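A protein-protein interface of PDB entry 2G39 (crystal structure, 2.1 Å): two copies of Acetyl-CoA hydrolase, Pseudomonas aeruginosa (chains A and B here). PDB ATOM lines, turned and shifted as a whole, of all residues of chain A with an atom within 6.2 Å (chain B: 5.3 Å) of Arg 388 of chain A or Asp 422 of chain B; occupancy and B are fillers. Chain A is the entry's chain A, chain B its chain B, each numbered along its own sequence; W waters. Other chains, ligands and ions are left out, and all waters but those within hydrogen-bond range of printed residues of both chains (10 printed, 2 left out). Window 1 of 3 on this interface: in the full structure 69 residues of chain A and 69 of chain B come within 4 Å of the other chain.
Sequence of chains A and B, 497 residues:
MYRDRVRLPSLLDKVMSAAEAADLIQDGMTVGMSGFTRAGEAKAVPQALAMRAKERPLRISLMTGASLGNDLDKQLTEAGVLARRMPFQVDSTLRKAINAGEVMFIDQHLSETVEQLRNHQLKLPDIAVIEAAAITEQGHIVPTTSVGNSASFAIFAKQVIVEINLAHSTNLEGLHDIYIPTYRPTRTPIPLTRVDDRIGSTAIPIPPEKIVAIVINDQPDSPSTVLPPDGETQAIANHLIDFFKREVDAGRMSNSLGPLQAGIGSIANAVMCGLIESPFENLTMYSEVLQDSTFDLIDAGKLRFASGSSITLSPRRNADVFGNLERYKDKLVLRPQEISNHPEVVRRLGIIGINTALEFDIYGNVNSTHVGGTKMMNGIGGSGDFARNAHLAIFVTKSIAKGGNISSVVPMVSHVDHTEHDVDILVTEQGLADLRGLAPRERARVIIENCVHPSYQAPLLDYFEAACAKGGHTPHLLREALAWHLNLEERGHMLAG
O of Gly 384 of chain A is in hydrogen-bond range of NH1 of Arg 388 of chain B (2.9 Å). The backbone carbonyl oxygen of Arg 388 of chain B lies close to the side-chain carboxylate of Glu 112 of chain A (3.3 Å). The side-chain carboxylate of Asp 422 of chain B is in salt-bridge range of the guanidinium group of Arg 388 of chain A (3.7 Å). The guanidinium group (NH1) of Arg 388 of chain A is in hydrogen-bond range of the backbone carbonyl oxygen (O) of Gly 384 of chain B (2.8 Å). The side-chain carboxylate of Asp 422 of chain A is in salt-bridge range of the guanidinium group of Arg 388 of chain B (3.7 Å). The backbone carbonyl oxygen of Arg 388 of chain A lies close to the side-chain carboxylate of Glu 112 of chain B, at 3.2 Å.
ND1 of His 109 of chain A lies within hydrogen-bond range of OE1 of Glu 112 of chain A (3.5 Å). NE of Arg 388 of chain B is in salt-bridge range of OD1 of Asp 422 of chain B (3.0 Å). OE1 of Glu 420 of chain B sits close to NE2 of His 421 of chain B (3.3 Å). A ring nitrogen (ND1) of His 109 of chain B lies within hydrogen-bond range of the side-chain carboxylate of Glu 112 of chain B, 3.4 Å away. The side-chain carboxylate (OD2) of Asp 422 of chain A is in salt-bridge range of the guanidinium group (NE) of Arg 388 of chain A, at 3.0 Å. N of His 421 of chain A sits close to OG1 of Thr 419 of chain A, 3.2 Å away.
Arg 388 of chain B touches His 109 of chain A. His 109 of chain A touches His 421 of chain B. His 109 of chain A touches Asp 422 of chain B. Arg 388 of chain B touches Asp 385 of chain A. NE of Arg 388 of chain A touches CE1 of His 109 of chain B, at 3.3 Å. Arg 388 of chain A touches Asp 385 of chain B. Arg 388 of chain A touches Arg 388 of chain B. His 109 of chain B touches His 421 of chain A. Asp 422 of chain A touches His 109 of chain B.
Of the printed residues of chain B, Glu 112 of chain A touches Arg 388. Arg 388 of chain A touches six residues of chain B. Printed residues of chain B within 4 Å of Asp 422 of chain A: His 109 and Arg 388. Printed residues of chain A within 4 Å of Gly 384 of chain B: Arg 388. Of the printed residues of chain A, Asp 385 of chain B touches Arg 388. Printed residues of chain A within 4 Å of Arg 388 of chain B: His 109, Glu 112, Gly 384, Asp 385, Arg 388 and Asp 422. Asp 422 of chain B touches two residues of chain A. The nearest residue of chain A that does not touch Asp 422 of chain B is Glu 112 of chain A (5.0 Å). The nearest printed residue of chain B that does not touch Asp 422 of chain A is Glu 112 of chain B (4.8 Å).
Of the 16 printed residues of chain A, 7 touch a printed residue of chain B. Printed residues of chain A that touch a printed residue of chain B: His 109, Glu 112, Gly 384, Asp 385, Arg 388, His 421 and Asp 422. Along chain A the printed residues that touch a printed residue of chain B span positions 109 to 422. Of the 16 printed residues of chain B, 7 touch a printed residue of chain A. Hydrophobic or aromatic side chains of chain B that line the printed part of chain A: His 109 and His 421. Among the printed residues, 15 pairs touch across the chains. Among the printed residues, Asp or Glu carboxylates within 4 Å of a Lys or Arg side-chain nitrogen of the other chain: Arg 388 of chain A with Asp 422 of chain B (3.7 Å) and Asp 422 of chain A with Arg 388 of chain B (3.7 Å).
His 109 of chain A touches Arg 388 of chain B, and with the chains exchanged Arg 388 of chain A touches His 109 of chain B. His 109 of chain A touches His 421 of chain B, and with the chains exchanged His 421 of chain A touches His 109 of chain B. Gly 384 of chain A touches Arg 388 of chain B, and with the chains exchanged Arg 388 of chain A touches Gly 384 of chain B. Arg 388 of chain A touches Asp 422 of chain B, and with the chains exchanged Asp 422 of chain A touches Arg 388 of chain B. Of the 15 pairs that touch across the chains among the printed residues, 15 have their exchanged pair printed and touching as well.
Water W3 lies within hydrogen-bond range of the side-chain carboxylate (OD1) of Asp 385 of chain A (2.6 Å), the side-chain carboxylate (OE2) of Glu 112 of chain A (2.8 Å) and the guanidinium group (NH1) of Arg 388 of chain B (3.2 Å). Water W1 lies within hydrogen-bond range of OD2 of Asp 422 of chain B (2.7 Å) and NH2 of Arg 388 of chain A (2.7 Å). Water W6 lies within hydrogen-bond range of ND2 of Asn 389 of chain A, OE2 of Glu 112 of chain B and O of Arg 388 of chain A. Water W4 lies within hydrogen-bond range of OD1 of Asn 389 of chain B, ND2 of Asn 389 of chain A and NH1 of Arg 388 of chain A. Water W5 lies within hydrogen-bond range of the side-chain carboxylate of Asp 385 of chain B (2.7 Å), the side-chain carboxylate of Glu 112 of chain B (2.8 Å) and the guanidinium group of Arg 388 of chain A (3.1 Å). Water W9 bridges ND2 of Asn 389 of chain B (2.8 Å) and OE2 of Glu 112 of chain A (2.9 Å).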
ATOM      1  N   HIS A 109      17.762 -38.276  -3.979  1.00  0.00           N
ATOM      2  CA  HIS A 109      17.014 -38.112  -5.202  1.00  0.00           C
ATOM      3  C   HIS A 109      17.285 -39.333  -6.045  1.00  0.00           C
ATOM      4  O   HIS A 109      18.460 -39.673  -6.273  1.00  0.00           O
ATOM      5  CB  HIS A 109      17.474 -36.895  -5.972  1.00  0.00           C
ATOM      6  CG  HIS A 109      17.097 -35.601  -5.334  1.00  0.00           C
ATOM      7  ND1 HIS A 109      18.005 -34.573  -5.135  1.00  0.00           N
ATOM      8  CD2 HIS A 109      15.910 -35.144  -4.894  1.00  0.00           C
ATOM      9  CE1 HIS A 109      17.385 -33.543  -4.583  1.00  0.00           C
ATOM     10  NE2 HIS A 109      16.112 -33.865  -4.432  1.00  0.00           N
ATOM     11  N   GLU A 112      20.052 -39.752  -8.732  1.00  0.00           N
ATOM     12  CA  GLU A 112      21.398 -39.226  -8.451  1.00  0.00           C
ATOM     13  C   GLU A 112      22.378 -40.236  -7.875  1.00  0.00           C
ATOM     14  O   GLU A 112      23.562 -40.024  -7.990  1.00  0.00           O
ATOM     15  CB  GLU A 112      21.342 -37.977  -7.548  1.00  0.00           C
ATOM     16  CG  GLU A 112      20.682 -36.754  -8.286  1.00  0.00           C
ATOM     17  CD  GLU A 112      20.607 -35.478  -7.455  1.00  0.00           C
ATOM     18  OE1 GLU A 112      21.155 -35.487  -6.311  1.00  0.00           O
ATOM     19  OE2 GLU A 112      20.059 -34.462  -8.003  1.00  0.00           O
ATOM     20  N   VAL A 346      13.715 -34.744 -18.082  1.00  0.00           N
ATOM     21  CA  VAL A 346      12.491 -34.195 -17.525  1.00  0.00           C
ATOM     22  C   VAL A 346      12.215 -32.811 -18.087  1.00  0.00           C
ATOM     23  O   VAL A 346      11.102 -32.513 -18.534  1.00  0.00           O
ATOM     24  CB  VAL A 346      12.537 -34.176 -15.967  1.00  0.00           C
ATOM     25  CG1 VAL A 346      11.324 -33.451 -15.408  1.00  0.00           C
ATOM     26  CG2 VAL A 346      12.571 -35.620 -15.431  1.00  0.00           C
ATOM     27  N   SER A 383      10.356 -37.586  -6.379  1.00  0.00           N
ATOM     28  CA  SER A 383       9.545 -36.378  -6.376  1.00  0.00           C
ATOM     29  C   SER A 383      10.358 -35.088  -6.692  1.00  0.00           C
ATOM     30  O   SER A 383       9.869 -34.166  -7.359  1.00  0.00           O
ATOM     31  CB  SER A 383       8.761 -36.221  -5.055  1.00  0.00           C
ATOM     32  OG  SER A 383       9.652 -36.010  -3.933  1.00  0.00           O
ATOM     33  N   GLY A 384      11.588 -35.029  -6.200  1.00  0.00           N
ATOM     34  CA  GLY A 384      12.447 -33.864  -6.427  1.00  0.00           C
ATOM     35  C   GLY A 384      13.029 -33.870  -7.840  1.00  0.00           C
ATOM     36  O   GLY A 384      13.127 -32.815  -8.482  1.00  0.00           O
ATOM     37  N   ASP A 385      13.439 -35.035  -8.341  1.00  0.00           N
ATOM     38  CA  ASP A 385      13.827 -35.139  -9.759  1.00  0.00           C
ATOM     39  C   ASP A 385      12.732 -34.572 -10.668  1.00  0.00           C
ATOM     40  O   ASP A 385      13.033 -33.834 -11.592  1.00  0.00           O
ATOM     41  CB  ASP A 385      14.066 -36.583 -10.189  1.00  0.00           C
ATOM     42  CG  ASP A 385      15.285 -37.195  -9.564  1.00  0.00           C
ATOM     43  OD1 ASP A 385      16.319 -36.496  -9.382  1.00  0.00           O
ATOM     44  OD2 ASP A 385      15.201 -38.410  -9.282  1.00  0.00           O
ATOM     45  N   PHE A 386      11.468 -34.921 -10.430  1.00  0.00           N
ATOM     46  CA  PHE A 386      10.403 -34.444 -11.332  1.00  0.00           C
ATOM     47  C   PHE A 386       9.996 -33.028 -11.008  1.00  0.00           C
ATOM     48  O   PHE A 386       9.970 -32.196 -11.921  1.00  0.00           O
ATOM     49  CB  PHE A 386       9.222 -35.396 -11.376  1.00  0.00           C
ATOM     50  CG  PHE A 386       9.568 -36.698 -12.025  1.00  0.00           C
ATOM     51  CD1 PHE A 386       9.639 -36.793 -13.437  1.00  0.00           C
ATOM     52  CD2 PHE A 386       9.898 -37.807 -11.256  1.00  0.00           C
ATOM     53  CE1 PHE A 386      10.004 -38.013 -14.066  1.00  0.00           C
ATOM     54  CE2 PHE A 386      10.250 -39.015 -11.880  1.00  0.00           C
ATOM     55  CZ  PHE A 386      10.307 -39.117 -13.278  1.00  0.00           C
ATOM     56  N   ALA A 387       9.749 -32.725  -9.722  1.00  0.00           N
ATOM     57  CA  ALA A 387       9.257 -31.373  -9.359  1.00  0.00           C
ATOM     58  C   ALA A 387      10.173 -30.240  -9.779  1.00  0.00           C
ATOM     59  O   ALA A 387       9.709 -29.227 -10.264  1.00  0.00           O
ATOM     60  CB  ALA A 387       8.894 -31.247  -7.853  1.00  0.00           C
ATOM     61  N   ARG A 388      11.464 -30.380  -9.545  1.00  0.00           N
ATOM     62  CA  ARG A 388      12.392 -29.316  -9.899  1.00  0.00           C
ATOM     63  C   ARG A 388      12.330 -28.952 -11.401  1.00  0.00           C
ATOM     64  O   ARG A 388      12.426 -27.768 -11.773  1.00  0.00           O
ATOM     65  CB  ARG A 388      13.821 -29.702  -9.495  1.00  0.00           C
ATOM     66  CG  ARG A 388      14.892 -28.703 -10.000  1.00  0.00           C
ATOM     67  CD  ARG A 388      14.780 -27.287  -9.350  1.00  0.00           C
ATOM     68  NE  ARG A 388      15.286 -27.232  -7.974  1.00  0.00           N
ATOM     69  CZ  ARG A 388      16.530 -26.913  -7.658  1.00  0.00           C
ATOM     70  NH1 ARG A 388      17.410 -26.626  -8.621  1.00  0.00           N
ATOM     71  NH2 ARG A 388      16.912 -26.893  -6.388  1.00  0.00           N
ATOM     72  N   ASN A 389      12.154 -29.959 -12.263  1.00  0.00           N
ATOM     73  CA  ASN A 389      12.400 -29.777 -13.684  1.00  0.00           C
ATOM     74  C   ASN A 389      11.170 -29.897 -14.563  1.00  0.00           C
ATOM     75  O   ASN A 389      11.259 -29.768 -15.803  1.00  0.00           O
ATOM     76  CB  ASN A 389      13.473 -30.754 -14.143  1.00  0.00           C
ATOM     77  CG  ASN A 389      14.751 -30.613 -13.351  1.00  0.00           C
ATOM     78  OD1 ASN A 389      15.157 -31.526 -12.597  1.00  0.00           O
ATOM     79  ND2 ASN A 389      15.370 -29.479 -13.475  1.00  0.00           N
ATOM     80  N   ALA A 390      10.033 -30.113 -13.910  1.00  0.00           N
ATOM     81  CA  ALA A 390       8.782 -30.342 -14.560  1.00  0.00           C
ATOM     82  C   ALA A 390       8.265 -29.063 -15.182  1.00  0.00           C
ATOM     83  O   ALA A 390       8.569 -27.945 -14.708  1.00  0.00           O
ATOM     84  CB  ALA A 390       7.723 -30.890 -13.519  1.00  0.00           C
ATOM     85  N   ALA A 393       4.724 -28.871 -11.722  1.00  0.00           N
ATOM     86  CA  ALA A 393       4.926 -29.666 -10.504  1.00  0.00           C
ATOM     87  C   ALA A 393       3.675 -29.538  -9.639  1.00  0.00           C
ATOM     88  O   ALA A 393       3.380 -28.469  -9.079  1.00  0.00           O
ATOM     89  CB  ALA A 393       6.167 -29.189  -9.753  1.00  0.00           C
ATOM     90  N   HIS A 418      10.613 -29.991  -0.837  1.00  0.00           N
ATOM     91  CA  HIS A 418      10.506 -29.156  -2.014  1.00  0.00           C
ATOM     92  C   HIS A 418      10.250 -27.747  -1.541  1.00  0.00           C
ATOM     93  O   HIS A 418       9.232 -27.497  -0.890  1.00  0.00           O
ATOM     94  CB  HIS A 418       9.378 -29.683  -2.943  1.00  0.00           C
ATOM     95  CG  HIS A 418       9.522 -31.152  -3.206  1.00  0.00           C
ATOM     96  ND1 HIS A 418       8.795 -32.111  -2.528  1.00  0.00           N
ATOM     97  CD2 HIS A 418      10.403 -31.827  -3.978  1.00  0.00           C
ATOM     98  CE1 HIS A 418       9.194 -33.315  -2.908  1.00  0.00           C
ATOM     99  NE2 HIS A 418      10.186 -33.169  -3.765  1.00  0.00           N
ATOM    100  N   THR A 419      11.184 -26.848  -1.839  1.00  0.00           N
ATOM    101  CA  THR A 419      10.995 -25.462  -1.508  1.00  0.00           C
ATOM    102  C   THR A 419       9.900 -24.946  -2.423  1.00  0.00           C
ATOM    103  O   THR A 419       9.533 -25.586  -3.408  1.00  0.00           O
ATOM    104  CB  THR A 419      12.259 -24.581  -1.755  1.00  0.00           C
ATOM    105  OG1 THR A 419      12.412 -24.370  -3.167  1.00  0.00           O
ATOM    106  CG2 THR A 419      13.537 -25.169  -1.132  1.00  0.00           C
ATOM    107  N   HIS A 421       9.985 -22.882  -4.642  1.00  0.00           N
ATOM    108  CA  HIS A 421      10.533 -22.685  -6.010  1.00  0.00           C
ATOM    109  C   HIS A 421      10.213 -23.839  -6.962  1.00  0.00           C
ATOM    110  O   HIS A 421      10.217 -23.649  -8.190  1.00  0.00           O
ATOM    111  CB  HIS A 421      12.052 -22.484  -5.955  1.00  0.00           C
ATOM    112  CG  HIS A 421      12.462 -21.322  -5.116  1.00  0.00           C
ATOM    113  ND1 HIS A 421      12.326 -20.017  -5.539  1.00  0.00           N
ATOM    114  CD2 HIS A 421      12.958 -21.260  -3.853  1.00  0.00           C
ATOM    115  CE1 HIS A 421      12.758 -19.200  -4.587  1.00  0.00           C
ATOM    116  NE2 HIS A 421      13.142 -19.928  -3.552  1.00  0.00           N
ATOM    117  N   ASP A 422       9.915 -25.016  -6.406  1.00  0.00           N
ATOM    118  CA  ASP A 422       9.680 -26.238  -7.174  1.00  0.00           C
ATOM    119  C   ASP A 422       8.254 -26.738  -7.077  1.00  0.00           C
ATOM    120  O   ASP A 422       7.976 -27.926  -7.304  1.00  0.00           O
ATOM    121  CB  ASP A 422      10.608 -27.348  -6.687  1.00  0.00           C
ATOM    122  CG  ASP A 422      12.071 -27.025  -6.867  1.00  0.00           C
ATOM    123  OD1 ASP A 422      12.417 -26.145  -7.678  1.00  0.00           O
ATOM    124  OD2 ASP A 422      12.895 -27.670  -6.190  1.00  0.00           O
ATOM    125  N   HIS B 109      14.494 -19.618  -9.621  1.00  0.00           N
ATOM    126  CA  HIS B 109      15.763 -20.184 -10.032  1.00  0.00           C
ATOM    127  C   HIS B 109      16.104 -19.461 -11.312  1.00  0.00           C
ATOM    128  O   HIS B 109      15.250 -19.371 -12.205  1.00  0.00           O
ATOM    129  CB  HIS B 109      15.667 -21.682 -10.314  1.00  0.00           C
ATOM    130  CG  HIS B 109      15.476 -22.507  -9.091  1.00  0.00           C
ATOM    131  ND1 HIS B 109      14.459 -23.431  -8.973  1.00  0.00           N
ATOM    132  CD2 HIS B 109      16.155 -22.530  -7.919  1.00  0.00           C
ATOM    133  CE1 HIS B 109      14.542 -24.012  -7.785  1.00  0.00           C
ATOM    134  NE2 HIS B 109      15.560 -23.480  -7.130  1.00  0.00           N
ATOM    135  N   GLU B 112      15.224 -20.719 -14.906  1.00  0.00           N
ATOM    136  CA  GLU B 112      13.852 -21.198 -15.119  1.00  0.00           C
ATOM    137  C   GLU B 112      12.858 -20.168 -15.671  1.00  0.00           C
ATOM    138  O   GLU B 112      11.903 -20.549 -16.332  1.00  0.00           O
ATOM    139  CB  GLU B 112      13.293 -21.861 -13.828  1.00  0.00           C
ATOM    140  CG  GLU B 112      14.060 -23.161 -13.531  1.00  0.00           C
ATOM    141  CD  GLU B 112      13.521 -23.973 -12.355  1.00  0.00           C
ATOM    142  OE1 GLU B 112      12.519 -23.532 -11.709  1.00  0.00           O
ATOM    143  OE2 GLU B 112      14.152 -25.052 -12.084  1.00  0.00           O
ATOM    144  N   GLY B 384      20.553 -22.608  -6.721  1.00  0.00           N
ATOM    145  CA  GLY B 384      19.761 -23.849  -6.814  1.00  0.00           C
ATOM    146  C   GLY B 384      19.977 -24.573  -8.133  1.00  0.00           C
ATOM    147  O   GLY B 384      20.071 -25.793  -8.164  1.00  0.00           O
ATOM    148  N   ASP B 385      20.016 -23.826  -9.228  1.00  0.00           N
ATOM    149  CA  ASP B 385      20.377 -24.417 -10.509  1.00  0.00           C
ATOM    150  C   ASP B 385      21.691 -25.200 -10.350  1.00  0.00           C
ATOM    151  O   ASP B 385      21.775 -26.339 -10.831  1.00  0.00           O
ATOM    152  CB  ASP B 385      20.582 -23.348 -11.605  1.00  0.00           C
ATOM    153  CG  ASP B 385      19.305 -22.630 -11.997  1.00  0.00           C
ATOM    154  OD1 ASP B 385      18.222 -23.268 -12.138  1.00  0.00           O
ATOM    155  OD2 ASP B 385      19.411 -21.407 -12.246  1.00  0.00           O
ATOM    156  N   ALA B 387      23.568 -26.046  -7.305  1.00  0.00           N
ATOM    157  CA  ALA B 387      23.684 -26.955  -6.184  1.00  0.00           C
ATOM    158  C   ALA B 387      23.002 -28.299  -6.457  1.00  0.00           C
ATOM    159  O   ALA B 387      23.559 -29.352  -6.144  1.00  0.00           O
ATOM    160  CB  ALA B 387      23.125 -26.339  -4.912  1.00  0.00           C
ATOM    161  N   ARG B 388      21.794 -28.243  -7.007  1.00  0.00           N
ATOM    162  CA  ARG B 388      21.019 -29.449  -7.299  1.00  0.00           C
ATOM    163  C   ARG B 388      21.789 -30.404  -8.227  1.00  0.00           C
ATOM    164  O   ARG B 388      21.805 -31.614  -8.013  1.00  0.00           O
ATOM    165  CB  ARG B 388      19.672 -29.074  -7.945  1.00  0.00           C
ATOM    166  CG  ARG B 388      18.832 -30.262  -8.436  1.00  0.00           C
ATOM    167  CD  ARG B 388      18.517 -31.256  -7.267  1.00  0.00           C
ATOM    168  NE  ARG B 388      17.349 -30.830  -6.470  1.00  0.00           N
ATOM    169  CZ  ARG B 388      16.081 -31.104  -6.761  1.00  0.00           C
ATOM    170  NH1 ARG B 388      15.755 -31.819  -7.843  1.00  0.00           N
ATOM    171  NH2 ARG B 388      15.121 -30.656  -5.968  1.00  0.00           N
ATOM    172  N   ASN B 389      22.436 -29.846  -9.247  1.00  0.00           N
ATOM    173  CA  ASN B 389      22.908 -30.660 -10.359  1.00  0.00           C
ATOM    174  C   ASN B 389      24.422 -30.809 -10.435  1.00  0.00           C
ATOM    175  O   ASN B 389      24.940 -31.554 -11.303  1.00  0.00           O
ATOM    176  CB  ASN B 389      22.357 -30.087 -11.669  1.00  0.00           C
ATOM    177  CG  ASN B 389      20.840 -30.055 -11.687  1.00  0.00           C
ATOM    178  OD1 ASN B 389      20.215 -28.972 -11.723  1.00  0.00           O
ATOM    179  ND2 ASN B 389      20.233 -31.231 -11.649  1.00  0.00           N
ATOM    180  N   ALA B 393      28.354 -29.700  -4.610  1.00  0.00           N
ATOM    181  CA  ALA B 393      27.654 -28.499  -4.173  1.00  0.00           C
ATOM    182  C   ALA B 393      28.279 -28.027  -2.843  1.00  0.00           C
ATOM    183  O   ALA B 393      28.051 -28.639  -1.795  1.00  0.00           O
ATOM    184  CB  ALA B 393      26.188 -28.808  -3.947  1.00  0.00           C
ATOM    185  N   PHE B 395      28.952 -24.989  -0.022  1.00  0.00           N
ATOM    186  CA  PHE B 395      28.417 -23.723   0.528  1.00  0.00           C
ATOM    187  C   PHE B 395      29.335 -23.191   1.585  1.00  0.00           C
ATOM    188  O   PHE B 395      29.866 -23.933   2.377  1.00  0.00           O
ATOM    189  CB  PHE B 395      26.986 -23.887   1.076  1.00  0.00           C
ATOM    190  CG  PHE B 395      25.923 -23.969   0.000  1.00  0.00           C
ATOM    191  CD1 PHE B 395      25.333 -22.819  -0.495  1.00  0.00           C
ATOM    192  CD2 PHE B 395      25.537 -25.191  -0.525  1.00  0.00           C
ATOM    193  CE1 PHE B 395      24.358 -22.870  -1.482  1.00  0.00           C
ATOM    194  CE2 PHE B 395      24.561 -25.265  -1.516  1.00  0.00           C
ATOM    195  CZ  PHE B 395      23.975 -24.110  -2.006  1.00  0.00           C
ATOM    196  N   HIS B 418      17.981 -24.541   0.051  1.00  0.00           N
ATOM    197  CA  HIS B 418      18.578 -25.793  -0.461  1.00  0.00           C
ATOM    198  C   HIS B 418      18.402 -26.862   0.571  1.00  0.00           C
ATOM    199  O   HIS B 418      18.877 -26.709   1.669  1.00  0.00           O
ATOM    200  CB  HIS B 418      20.070 -25.587  -0.791  1.00  0.00           C
ATOM    201  CG  HIS B 418      20.270 -24.457  -1.734  1.00  0.00           C
ATOM    202  ND1 HIS B 418      20.575 -23.185  -1.308  1.00  0.00           N
ATOM    203  CD2 HIS B 418      20.056 -24.373  -3.064  1.00  0.00           C
ATOM    204  CE1 HIS B 418      20.591 -22.369  -2.346  1.00  0.00           C
ATOM    205  NE2 HIS B 418      20.257 -23.060  -3.421  1.00  0.00           N
ATOM    206  N   THR B 419      17.677 -27.927   0.244  1.00  0.00           N
ATOM    207  CA  THR B 419      17.572 -29.037   1.197  1.00  0.00           C
ATOM    208  C   THR B 419      18.921 -29.734   1.280  1.00  0.00           C
ATOM    209  O   THR B 419      19.802 -29.553   0.417  1.00  0.00           O
ATOM    210  CB  THR B 419      16.482 -30.062   0.866  1.00  0.00           C
ATOM    211  OG1 THR B 419      16.990 -30.971  -0.111  1.00  0.00           O
ATOM    212  CG2 THR B 419      15.214 -29.360   0.291  1.00  0.00           C
ATOM    213  N   GLU B 420      19.065 -30.533   2.327  1.00  0.00           N
ATOM    214  CA  GLU B 420      20.285 -31.283   2.538  1.00  0.00           C
ATOM    215  C   GLU B 420      20.606 -32.268   1.388  1.00  0.00           C
ATOM    216  O   GLU B 420      21.750 -32.629   1.191  1.00  0.00           O
ATOM    217  CB  GLU B 420      20.232 -31.970   3.911  1.00  0.00           C
ATOM    218  CG  GLU B 420      19.113 -32.907   4.085  1.00  0.00           C
ATOM    219  CD  GLU B 420      19.442 -34.245   3.493  1.00  0.00           C
ATOM    220  OE1 GLU B 420      18.488 -34.998   3.201  1.00  0.00           O
ATOM    221  OE2 GLU B 420      20.657 -34.527   3.267  1.00  0.00           O
ATOM    222  N   HIS B 421      19.598 -32.640   0.607  1.00  0.00           N
ATOM    223  CA  HIS B 421      19.812 -33.394  -0.635  1.00  0.00           C
ATOM    224  C   HIS B 421      20.666 -32.680  -1.663  1.00  0.00           C
ATOM    225  O   HIS B 421      21.243 -33.353  -2.511  1.00  0.00           O
ATOM    226  CB  HIS B 421      18.485 -33.717  -1.280  1.00  0.00           C
ATOM    227  CG  HIS B 421      17.564 -34.456  -0.380  1.00  0.00           C
ATOM    228  ND1 HIS B 421      17.718 -35.800  -0.110  1.00  0.00           N
ATOM    229  CD2 HIS B 421      16.498 -34.043   0.348  1.00  0.00           C
ATOM    230  CE1 HIS B 421      16.747 -36.196   0.696  1.00  0.00           C
ATOM    231  NE2 HIS B 421      16.017 -35.144   1.021  1.00  0.00           N
ATOM    232  N   ASP B 422      20.750 -31.332  -1.605  1.00  0.00           N
ATOM    233  CA  ASP B 422      21.541 -30.567  -2.602  1.00  0.00           C
ATOM    234  C   ASP B 422      22.825 -29.946  -2.075  1.00  0.00           C
ATOM    235  O   ASP B 422      23.338 -28.975  -2.651  1.00  0.00           O
ATOM    236  CB  ASP B 422      20.681 -29.481  -3.239  1.00  0.00           C
ATOM    237  CG  ASP B 422      19.413 -30.040  -3.870  1.00  0.00           C
ATOM    238  OD1 ASP B 422      19.358 -31.243  -4.249  1.00  0.00           O
ATOM    239  OD2 ASP B 422      18.460 -29.276  -3.950  1.00  0.00           O
ATOM    240  N   VAL B 423      23.306 -30.474  -0.949  1.00  0.00           N
ATOM    241  CA  VAL B 423      24.442 -29.864  -0.245  1.00  0.00           C
ATOM    242  C   VAL B 423      25.459 -30.959   0.062  1.00  0.00           C
ATOM    243  O   VAL B 423      25.154 -31.903   0.790  1.00  0.00           O
ATOM    244  CB  VAL B 423      24.003 -29.170   1.046  1.00  0.00           C
ATOM    245  CG1 VAL B 423      25.216 -28.588   1.773  1.00  0.00           C
ATOM    246  CG2 VAL B 423      22.939 -28.100   0.771  1.00  0.00           C
ATOM    247  N   ASP B 424      26.665 -30.834  -0.499  1.00  0.00           N
ATOM    248  CA  ASP B 424      27.664 -31.867  -0.303  1.00  0.00           C
ATOM    249  C   ASP B 424      28.684 -31.474   0.745  1.00  0.00           C
ATOM    250  O   ASP B 424      29.141 -32.304   1.482  1.00  0.00           O
ATOM    251  CB  ASP B 424      28.348 -32.173  -1.618  1.00  0.00           C
ATOM    252  CG  ASP B 424      27.367 -32.599  -2.668  1.00  0.00           C
ATOM    253  OD1 ASP B 424      26.520 -33.447  -2.350  1.00  0.00           O
ATOM    254  OD2 ASP B 424      27.422 -32.091  -3.801  1.00  0.00           O
HETATM  255  O   HOH W   1      18.962 -26.685  -4.584  1.00  0.00           O
HETATM  256  O   HOH W   2      11.744 -21.153  -9.933  1.00  0.00           O
HETATM  257  O   HOH W   3      17.534 -34.150  -9.178  1.00  0.00           O
HETATM  258  O   HOH W   4      17.573 -28.249 -11.587  1.00  0.00           O
HETATM  259  O   HOH W   5      16.860 -25.555 -11.463  1.00  0.00           O
HETATM  260  O   HOH W   6      14.769 -26.914 -14.150  1.00  0.00           O
HETATM  261  O   HOH W   7      12.362 -30.532  -5.637  1.00  0.00           O
HETATM  262  O   HOH W   8      16.497 -30.985  -2.707  1.00  0.00           O
HETATM  263  O   HOH W   9      20.862 -33.837 -10.740  1.00  0.00           O
HETATM  264  O   HOH W  10      17.478 -31.895 -10.938  1.00  0.00           O
